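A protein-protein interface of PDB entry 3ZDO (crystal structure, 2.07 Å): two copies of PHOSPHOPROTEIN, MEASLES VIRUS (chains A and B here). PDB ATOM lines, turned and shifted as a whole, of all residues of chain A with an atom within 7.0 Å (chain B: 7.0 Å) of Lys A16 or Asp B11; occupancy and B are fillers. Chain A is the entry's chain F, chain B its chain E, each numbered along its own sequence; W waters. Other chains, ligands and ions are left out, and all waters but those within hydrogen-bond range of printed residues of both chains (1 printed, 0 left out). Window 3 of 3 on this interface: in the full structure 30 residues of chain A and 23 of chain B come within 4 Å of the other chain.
CZ of Phe A9 touches OE2 of Glu B7, at 3.1 Å. Phe A9 touches Asp B11 (CZ to OD2, 3.3 Å). CD1 of Ile B15 touches CG1 of Val A12 (3.8 Å). OE1 of Gln A13 touches OD2 of Asp B11, at 3.5 Å. Ile B15 touches Ile A15 (CD1 to CG2, 3.9 Å). CG1 of Ile B15 touches CG of Lys A16, 3.8 Å away. Leu A19 touches Ile B15 (CD1 to CG2, 3.8 Å).
Printed residues of chain B within 4 Å of Phe A9: Glu B7 (3.1 Å) and Asp B11 (3.3 Å). Of the printed residues of chain B, Val A12 touches Ile B15 (3.8 Å). Printed residues of chain B within 4 Å of Ile A15: Ile B15. Lys A16 touches just these residues of chain B: Asp B11, Asp B14 and Ile B15. Thr A17 touches none of the printed residues of chain B. Of the printed residues of chain B, Leu A19 touches Ile B15 (3.8 Å). Asp B6 touches none of the printed residues of chain A. Of chain A, only Phe A9, Gln A13 and Lys A16 come within 4 Å of Asp B11. Of the printed residues of chain A, Ile B15 touches Val A12 (3.8 Å), Ile A15 (3.9 Å), Lys A16 (3.8 Å) and Leu A19 (3.8 Å). The nearest residue of chain A that does not touch Asp B11 is Val A12 (4.3 Å).
Of the 12 printed residues of chain A, 6 touch a printed residue of chain B. Hydrophobic or aromatic side chains of chain A that line the printed part of chain B: Phe A9, Val A12, Ile A15 and Leu A19. Printed residues of chain B that touch a printed residue of chain A: Glu B7, Asp B11, Asp B14 and Ile B15. Hydrophobic or aromatic side chains of chain B within 4 Å of the printed part of chain A: Ile B15. Along chain B the printed residues that touch a printed residue of chain A span positions 7 to 15. Among the printed residues, Asp or Glu carboxylates within 4 Å of a Lys or Arg side-chain nitrogen of the other chain: Lys A16 with Asp B11 and Lys A16 with Asp B14.
The side-chain carboxylate (OD1) of Asp B11 is in salt-bridge range of the side-chain amino group (NZ) of Lys A16 (3.2 Å). The side-chain carboxylate of Asp B14 lies within salt-bridge range of the side-chain amino group of Lys A16, 2.4 Å away.
Phe A9 touches Asp B11, but with the chains exchanged Asp A11 does not touch Phe B9 (12.4 Å). Val A12 touches Ile B15, but with the chains exchanged Ile A15 does not touch Val B12 (7.6 Å). Ile A15 touches its own counterpart, Ile B15. Lys A16 touches Asp B11, but with the chains exchanged Asp A11 does not touch Lys B16 (11.9 Å). Positions printed for both chains: 9, 11, 12, 13, 14, 15, 16, 17 and 18. Of the 9 pairs that touch across the chains among the printed residues, 1 has its exchanged pair printed and touching as well.
Water W1 bridges O of Leu A19 and O of Ala B18.
The side-chain hydroxyl (OG) of Ser B10 is in hydrogen-bond range of the backbone carbonyl oxygen (O) of Glu B7, 2.6 Å away. The side-chain hydroxyl (OG1) of Thr A17 sits at hydrogen-bond distance from the backbone carbonyl oxygen (O) of Gln A13, 2.9 Å away.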
ATOM      1  N   PHE A   9      11.560  15.037  14.446  1.00  0.00           N
ATOM      2  CA  PHE A   9      11.478  14.973  13.000  1.00  0.00           C
ATOM      3  C   PHE A   9      12.753  15.511  12.345  1.00  0.00           C
ATOM      4  O   PHE A   9      13.253  14.937  11.377  1.00  0.00           O
ATOM      5  CB  PHE A   9      10.223  15.680  12.478  1.00  0.00           C
ATOM      6  CG  PHE A   9       9.525  14.916  11.393  1.00  0.00           C
ATOM      7  CD1 PHE A   9       8.806  13.752  11.696  1.00  0.00           C
ATOM      8  CD2 PHE A   9       9.626  15.315  10.054  1.00  0.00           C
ATOM      9  CE1 PHE A   9       8.179  13.024  10.686  1.00  0.00           C
ATOM     10  CE2 PHE A   9       9.001  14.591   9.041  1.00  0.00           C
ATOM     11  CZ  PHE A   9       8.278  13.446   9.358  1.00  0.00           C
ATOM     12  N   ASP A  11      15.705  15.337  13.661  1.00  0.00           N
ATOM     13  CA  ASP A  11      16.683  14.269  13.941  1.00  0.00           C
ATOM     14  C   ASP A  11      16.587  13.103  12.973  1.00  0.00           C
ATOM     15  O   ASP A  11      17.605  12.581  12.528  1.00  0.00           O
ATOM     16  CB  ASP A  11      16.472  13.707  15.358  1.00  0.00           C
ATOM     17  CG  ASP A  11      17.106  14.553  16.424  1.00  0.00           C
ATOM     18  OD1 ASP A  11      17.892  15.471  16.085  1.00  0.00           O
ATOM     19  OD2 ASP A  11      16.830  14.294  17.617  1.00  0.00           O
ATOM     20  N   VAL A  12      15.351  12.691  12.686  1.00  0.00           N
ATOM     21  CA  VAL A  12      15.048  11.555  11.821  1.00  0.00           C
ATOM     22  C   VAL A  12      15.452  11.853  10.372  1.00  0.00           C
ATOM     23  O   VAL A  12      15.917  10.947   9.630  1.00  0.00           O
ATOM     24  CB  VAL A  12      13.540  11.224  11.875  1.00  0.00           C
ATOM     25  CG1 VAL A  12      13.308   9.730  11.819  1.00  0.00           C
ATOM     26  CG2 VAL A  12      12.942  11.766  13.167  1.00  0.00           C
ATOM     27  N   GLN A  13      15.317  13.122   9.987  1.00  0.00           N
ATOM     28  CA  GLN A  13      15.777  13.561   8.683  1.00  0.00           C
ATOM     29  C   GLN A  13      17.300  13.700   8.648  1.00  0.00           C
ATOM     30  O   GLN A  13      17.903  13.567   7.592  1.00  0.00           O
ATOM     31  CB  GLN A  13      15.097  14.878   8.259  1.00  0.00           C
ATOM     32  CG  GLN A  13      13.574  14.786   8.092  1.00  0.00           C
ATOM     33  CD  GLN A  13      13.154  14.008   6.855  1.00  0.00           C
ATOM     34  OE1 GLN A  13      12.437  13.002   6.950  1.00  0.00           O
ATOM     35  NE2 GLN A  13      13.612  14.457   5.686  1.00  0.00           N
ATOM     36  N   ASP A  14      17.923  13.971   9.789  1.00  0.00           N
ATOM     37  CA  ASP A  14      19.395  13.958   9.843  1.00  0.00           C
ATOM     38  C   ASP A  14      20.013  12.568   9.678  1.00  0.00           C
ATOM     39  O   ASP A  14      21.118  12.448   9.168  1.00  0.00           O
ATOM     40  CB  ASP A  14      19.902  14.550  11.142  1.00  0.00           C
ATOM     41  CG  ASP A  14      19.963  16.035  11.106  1.00  0.00           C
ATOM     42  OD1 ASP A  14      18.944  16.655  10.745  1.00  0.00           O
ATOM     43  OD2 ASP A  14      21.037  16.590  11.431  1.00  0.00           O
ATOM     44  N   ILE A  15      19.318  11.542  10.169  1.00  0.00           N
ATOM     45  CA  ILE A  15      19.770  10.151  10.048  1.00  0.00           C
ATOM     46  C   ILE A  15      19.674   9.720   8.597  1.00  0.00           C
ATOM     47  O   ILE A  15      20.621   9.155   8.057  1.00  0.00           O
ATOM     48  CB  ILE A  15      18.936   9.200  10.936  1.00  0.00           C
ATOM     49  CG1 ILE A  15      19.216   9.505  12.415  1.00  0.00           C
ATOM     50  CG2 ILE A  15      19.210   7.717  10.597  1.00  0.00           C
ATOM     51  CD1 ILE A  15      18.223   8.844  13.349  1.00  0.00           C
ATOM     52  N   LYS A  16      18.524  10.026   7.980  1.00  0.00           N
ATOM     53  CA  LYS A  16      18.254   9.775   6.559  1.00  0.00           C
ATOM     54  C   LYS A  16      19.292  10.376   5.619  1.00  0.00           C
ATOM     55  O   LYS A  16      19.734   9.707   4.679  1.00  0.00           O
ATOM     56  CB  LYS A  16      16.834  10.257   6.163  1.00  0.00           C
ATOM     57  CG  LYS A  16      15.754   9.220   6.423  1.00  0.00           C
ATOM     58  CD  LYS A  16      14.331   9.786   6.415  1.00  0.00           C
ATOM     59  CE  LYS A  16      13.755   9.821   5.007  1.00  0.00           C
ATOM     60  NZ  LYS A  16      12.289   9.593   5.069  1.00  0.00           N
ATOM     61  N   THR A  17      19.650  11.635   5.880  1.00  0.00           N
ATOM     62  CA  THR A  17      20.645  12.375   5.102  1.00  0.00           C
ATOM     63  C   THR A  17      22.121  11.899   5.304  1.00  0.00           C
ATOM     64  O   THR A  17      22.900  11.965   4.378  1.00  0.00           O
ATOM     65  CB  THR A  17      20.560  13.886   5.403  1.00  0.00           C
ATOM     66  OG1 THR A  17      19.238  14.351   5.102  1.00  0.00           O
ATOM     67  CG2 THR A  17      21.548  14.639   4.563  1.00  0.00           C
ATOM     68  N   ALA A  18      22.510  11.536   6.522  1.00  0.00           N
ATOM     69  CA  ALA A  18      23.847  10.976   6.750  1.00  0.00           C
ATOM     70  C   ALA A  18      23.940   9.541   6.136  1.00  0.00           C
ATOM     71  O   ALA A  18      24.963   9.162   5.618  1.00  0.00           O
ATOM     72  CB  ALA A  18      24.170  10.968   8.247  1.00  0.00           C
ATOM     73  N   LEU A  19      22.870   8.761   6.227  1.00  0.00           N
ATOM     74  CA  LEU A  19      22.761   7.485   5.525  1.00  0.00           C
ATOM     75  C   LEU A  19      22.854   7.626   4.008  1.00  0.00           C
ATOM     76  O   LEU A  19      23.485   6.792   3.392  1.00  0.00           O
ATOM     77  CB  LEU A  19      21.450   6.776   5.891  1.00  0.00           C
ATOM     78  CG  LEU A  19      21.527   6.114   7.298  1.00  0.00           C
ATOM     79  CD1 LEU A  19      20.190   5.492   7.707  1.00  0.00           C
ATOM     80  CD2 LEU A  19      22.606   5.020   7.267  1.00  0.00           C
ATOM     81  N   ALA A  20      22.170   8.641   3.413  1.00  0.00           N
ATOM     82  CA  ALA A  20      22.306   8.940   1.997  1.00  0.00           C
ATOM     83  C   ALA A  20      23.746   9.394   1.650  1.00  0.00           C
ATOM     84  O   ALA A  20      24.282   9.072   0.573  1.00  0.00           O
ATOM     85  CB  ALA A  20      21.238   9.994   1.531  1.00  0.00           C
ATOM     86  N   LYS A  21      24.395  10.117   2.536  1.00  0.00           N
ATOM     87  CA  LYS A  21      25.778  10.574   2.253  1.00  0.00           C
ATOM     88  C   LYS A  21      26.823   9.409   2.340  1.00  0.00           C
ATOM     89  O   LYS A  21      27.791   9.393   1.592  1.00  0.00           O
ATOM     90  CB  LYS A  21      26.181  11.693   3.192  1.00  0.00           C
ATOM     91  CG  LYS A  21      27.660  12.095   3.084  1.00  0.00           C
ATOM     92  CD  LYS A  21      27.890  13.033   1.890  1.00  0.00           C
ATOM     93  CE  LYS A  21      29.258  12.857   1.255  1.00  0.00           C
ATOM     94  NZ  LYS A  21      29.685  14.066   0.482  1.00  0.00           N
ATOM     95  N   ASP B   6       1.422   6.198  10.806  1.00  0.00           N
ATOM     96  CA  ASP B   6       2.122   7.435  11.248  1.00  0.00           C
ATOM     97  C   ASP B   6       3.136   7.909  10.189  1.00  0.00           C
ATOM     98  O   ASP B   6       3.530   7.153   9.298  1.00  0.00           O
ATOM     99  CB  ASP B   6       2.815   7.192  12.598  1.00  0.00           C
ATOM    100  CG  ASP B   6       2.571   8.315  13.600  1.00  0.00           C
ATOM    101  OD1 ASP B   6       2.238   9.453  13.185  1.00  0.00           O
ATOM    102  OD2 ASP B   6       2.719   8.056  14.813  1.00  0.00           O
ATOM    103  N   GLU B   7       3.517   9.178  10.278  1.00  0.00           N
ATOM    104  CA  GLU B   7       4.590   9.742   9.474  1.00  0.00           C
ATOM    105  C   GLU B   7       5.908   9.053   9.889  1.00  0.00           C
ATOM    106  O   GLU B   7       6.746   8.698   9.048  1.00  0.00           O
ATOM    107  CB  GLU B   7       4.671  11.247   9.757  1.00  0.00           C
ATOM    108  CG  GLU B   7       4.791  12.158   8.541  1.00  0.00           C
ATOM    109  CD  GLU B   7       5.082  13.608   8.926  1.00  0.00           C
ATOM    110  OE1 GLU B   7       4.803  13.999  10.080  1.00  0.00           O
ATOM    111  OE2 GLU B   7       5.597  14.368   8.081  1.00  0.00           O
ATOM    112  N   LEU B   8       6.033   8.839  11.198  1.00  0.00           N
ATOM    113  CA  LEU B   8       7.211   8.280  11.848  1.00  0.00           C
ATOM    114  C   LEU B   8       7.529   6.840  11.417  1.00  0.00           C
ATOM    115  O   LEU B   8       8.667   6.550  11.076  1.00  0.00           O
ATOM    116  CB  LEU B   8       7.053   8.383  13.380  1.00  0.00           C
ATOM    117  CG  LEU B   8       8.109   7.786  14.318  1.00  0.00           C
ATOM    118  CD1 LEU B   8       9.408   8.579  14.275  1.00  0.00           C
ATOM    119  CD2 LEU B   8       7.581   7.710  15.745  1.00  0.00           C
ATOM    120  N   PHE B   9       6.530   5.954  11.436  1.00  0.00           N
ATOM    121  CA  PHE B   9       6.705   4.534  11.069  1.00  0.00           C
ATOM    122  C   PHE B   9       7.268   4.385   9.658  1.00  0.00           C
ATOM    123  O   PHE B   9       8.160   3.561   9.410  1.00  0.00           O
ATOM    124  CB  PHE B   9       5.377   3.753  11.208  1.00  0.00           C
ATOM    125  CG  PHE B   9       5.441   2.302  10.734  1.00  0.00           C
ATOM    126  CD1 PHE B   9       5.990   1.302  11.546  1.00  0.00           C
ATOM    127  CD2 PHE B   9       4.918   1.931   9.482  1.00  0.00           C
ATOM    128  CE1 PHE B   9       6.041  -0.022  11.109  1.00  0.00           C
ATOM    129  CE2 PHE B   9       4.968   0.610   9.048  1.00  0.00           C
ATOM    130  CZ  PHE B   9       5.523  -0.369   9.866  1.00  0.00           C
ATOM    131  N   SER B  10       6.737   5.181   8.739  1.00  0.00           N
ATOM    132  CA  SER B  10       7.169   5.132   7.361  1.00  0.00           C
ATOM    133  C   SER B  10       8.602   5.686   7.231  1.00  0.00           C
ATOM    134  O   SER B  10       9.409   5.142   6.472  1.00  0.00           O
ATOM    135  CB  SER B  10       6.221   5.950   6.512  1.00  0.00           C
ATOM    136  OG  SER B  10       6.305   7.298   6.928  1.00  0.00           O
ATOM    137  N   ASP B  11       8.911   6.763   7.965  1.00  0.00           N
ATOM    138  CA  ASP B  11      10.289   7.292   8.035  1.00  0.00           C
ATOM    139  C   ASP B  11      11.278   6.248   8.571  1.00  0.00           C
ATOM    140  O   ASP B  11      12.371   6.085   8.050  1.00  0.00           O
ATOM    141  CB  ASP B  11      10.369   8.548   8.914  1.00  0.00           C
ATOM    142  CG  ASP B  11      10.099   9.827   8.140  1.00  0.00           C
ATOM    143  OD1 ASP B  11       9.743   9.735   6.939  1.00  0.00           O
ATOM    144  OD2 ASP B  11      10.253  10.926   8.733  1.00  0.00           O
ATOM    145  N   VAL B  12      10.897   5.566   9.633  1.00  0.00           N
ATOM    146  CA  VAL B  12      11.749   4.496  10.165  1.00  0.00           C
ATOM    147  C   VAL B  12      11.933   3.356   9.154  1.00  0.00           C
ATOM    148  O   VAL B  12      13.030   2.790   9.039  1.00  0.00           O
ATOM    149  CB  VAL B  12      11.257   4.038  11.565  1.00  0.00           C
ATOM    150  CG1 VAL B  12      11.830   2.693  11.961  1.00  0.00           C
ATOM    151  CG2 VAL B  12      11.637   5.088  12.578  1.00  0.00           C
ATOM    152  N   GLN B  13      10.883   3.044   8.390  1.00  0.00           N
ATOM    153  CA  GLN B  13      11.005   2.109   7.242  1.00  0.00           C
ATOM    154  C   GLN B  13      12.023   2.583   6.192  1.00  0.00           C
ATOM    155  O   GLN B  13      12.709   1.760   5.576  1.00  0.00           O
ATOM    156  CB  GLN B  13       9.653   1.901   6.553  1.00  0.00           C
ATOM    157  CG  GLN B  13       8.562   1.321   7.448  1.00  0.00           C
ATOM    158  CD  GLN B  13       9.073   0.224   8.382  1.00  0.00           C
ATOM    159  OE1 GLN B  13       9.700  -0.741   7.936  1.00  0.00           O
ATOM    160  NE2 GLN B  13       8.803   0.371   9.686  1.00  0.00           N
ATOM    161  N   ASP B  14      12.051   3.896   5.954  1.00  0.00           N
ATOM    162  CA  ASP B  14      13.002   4.540   5.013  1.00  0.00           C
ATOM    163  C   ASP B  14      14.459   4.342   5.484  1.00  0.00           C
ATOM    164  O   ASP B  14      15.365   4.075   4.685  1.00  0.00           O
ATOM    165  CB  ASP B  14      12.761   6.058   4.955  1.00  0.00           C
ATOM    166  CG  ASP B  14      11.467   6.439   4.219  1.00  0.00           C
ATOM    167  OD1 ASP B  14      10.835   5.563   3.586  1.00  0.00           O
ATOM    168  OD2 ASP B  14      11.103   7.640   4.262  1.00  0.00           O
ATOM    169  N   ILE B  15      14.659   4.550   6.782  1.00  0.00           N
ATOM    170  CA  ILE B  15      15.945   4.321   7.448  1.00  0.00           C
ATOM    171  C   ILE B  15      16.414   2.855   7.338  1.00  0.00           C
ATOM    172  O   ILE B  15      17.570   2.595   6.975  1.00  0.00           O
ATOM    173  CB  ILE B  15      15.884   4.827   8.919  1.00  0.00           C
ATOM    174  CG1 ILE B  15      15.755   6.356   8.937  1.00  0.00           C
ATOM    175  CG2 ILE B  15      17.111   4.389   9.725  1.00  0.00           C
ATOM    176  CD1 ILE B  15      15.449   6.945  10.308  1.00  0.00           C
ATOM    177  N   LYS B  16      15.523   1.901   7.623  1.00  0.00           N
ATOM    178  CA  LYS B  16      15.818   0.464   7.399  1.00  0.00           C
ATOM    179  C   LYS B  16      16.216   0.148   5.936  1.00  0.00           C
ATOM    180  O   LYS B  16      17.201  -0.551   5.684  1.00  0.00           O
ATOM    181  CB  LYS B  16      14.620  -0.417   7.806  1.00  0.00           C
ATOM    182  CG  LYS B  16      14.153  -0.295   9.246  1.00  0.00           C
ATOM    183  CD  LYS B  16      14.562  -1.515  10.054  1.00  0.00           C
ATOM    184  CE  LYS B  16      13.884  -1.510  11.409  1.00  0.00           C
ATOM    185  NZ  LYS B  16      12.547  -2.158  11.350  1.00  0.00           N
ATOM    186  N   THR B  17      15.439   0.646   4.974  1.00  0.00           N
ATOM    187  CA  THR B  17      15.803   0.554   3.539  1.00  0.00           C
ATOM    188  C   THR B  17      17.189   1.148   3.234  1.00  0.00           C
ATOM    189  O   THR B  17      18.000   0.557   2.480  1.00  0.00           O
ATOM    190  CB  THR B  17      14.747   1.291   2.683  1.00  0.00           C
ATOM    191  OG1 THR B  17      13.466   0.739   2.967  1.00  0.00           O
ATOM    192  CG2 THR B  17      15.041   1.193   1.163  1.00  0.00           C
ATOM    193  N   ALA B  18      17.462   2.327   3.774  1.00  0.00           N
ATOM    194  CA  ALA B  18      18.738   2.963   3.458  1.00  0.00           C
ATOM    195  C   ALA B  18      19.904   2.205   4.132  1.00  0.00           C
ATOM    196  O   ALA B  18      20.977   2.065   3.563  1.00  0.00           O
ATOM    197  CB  ALA B  18      18.714   4.421   3.883  1.00  0.00           C
HETATM  198  O   HOH W   1      21.729   4.734   2.024  1.00  0.00           O
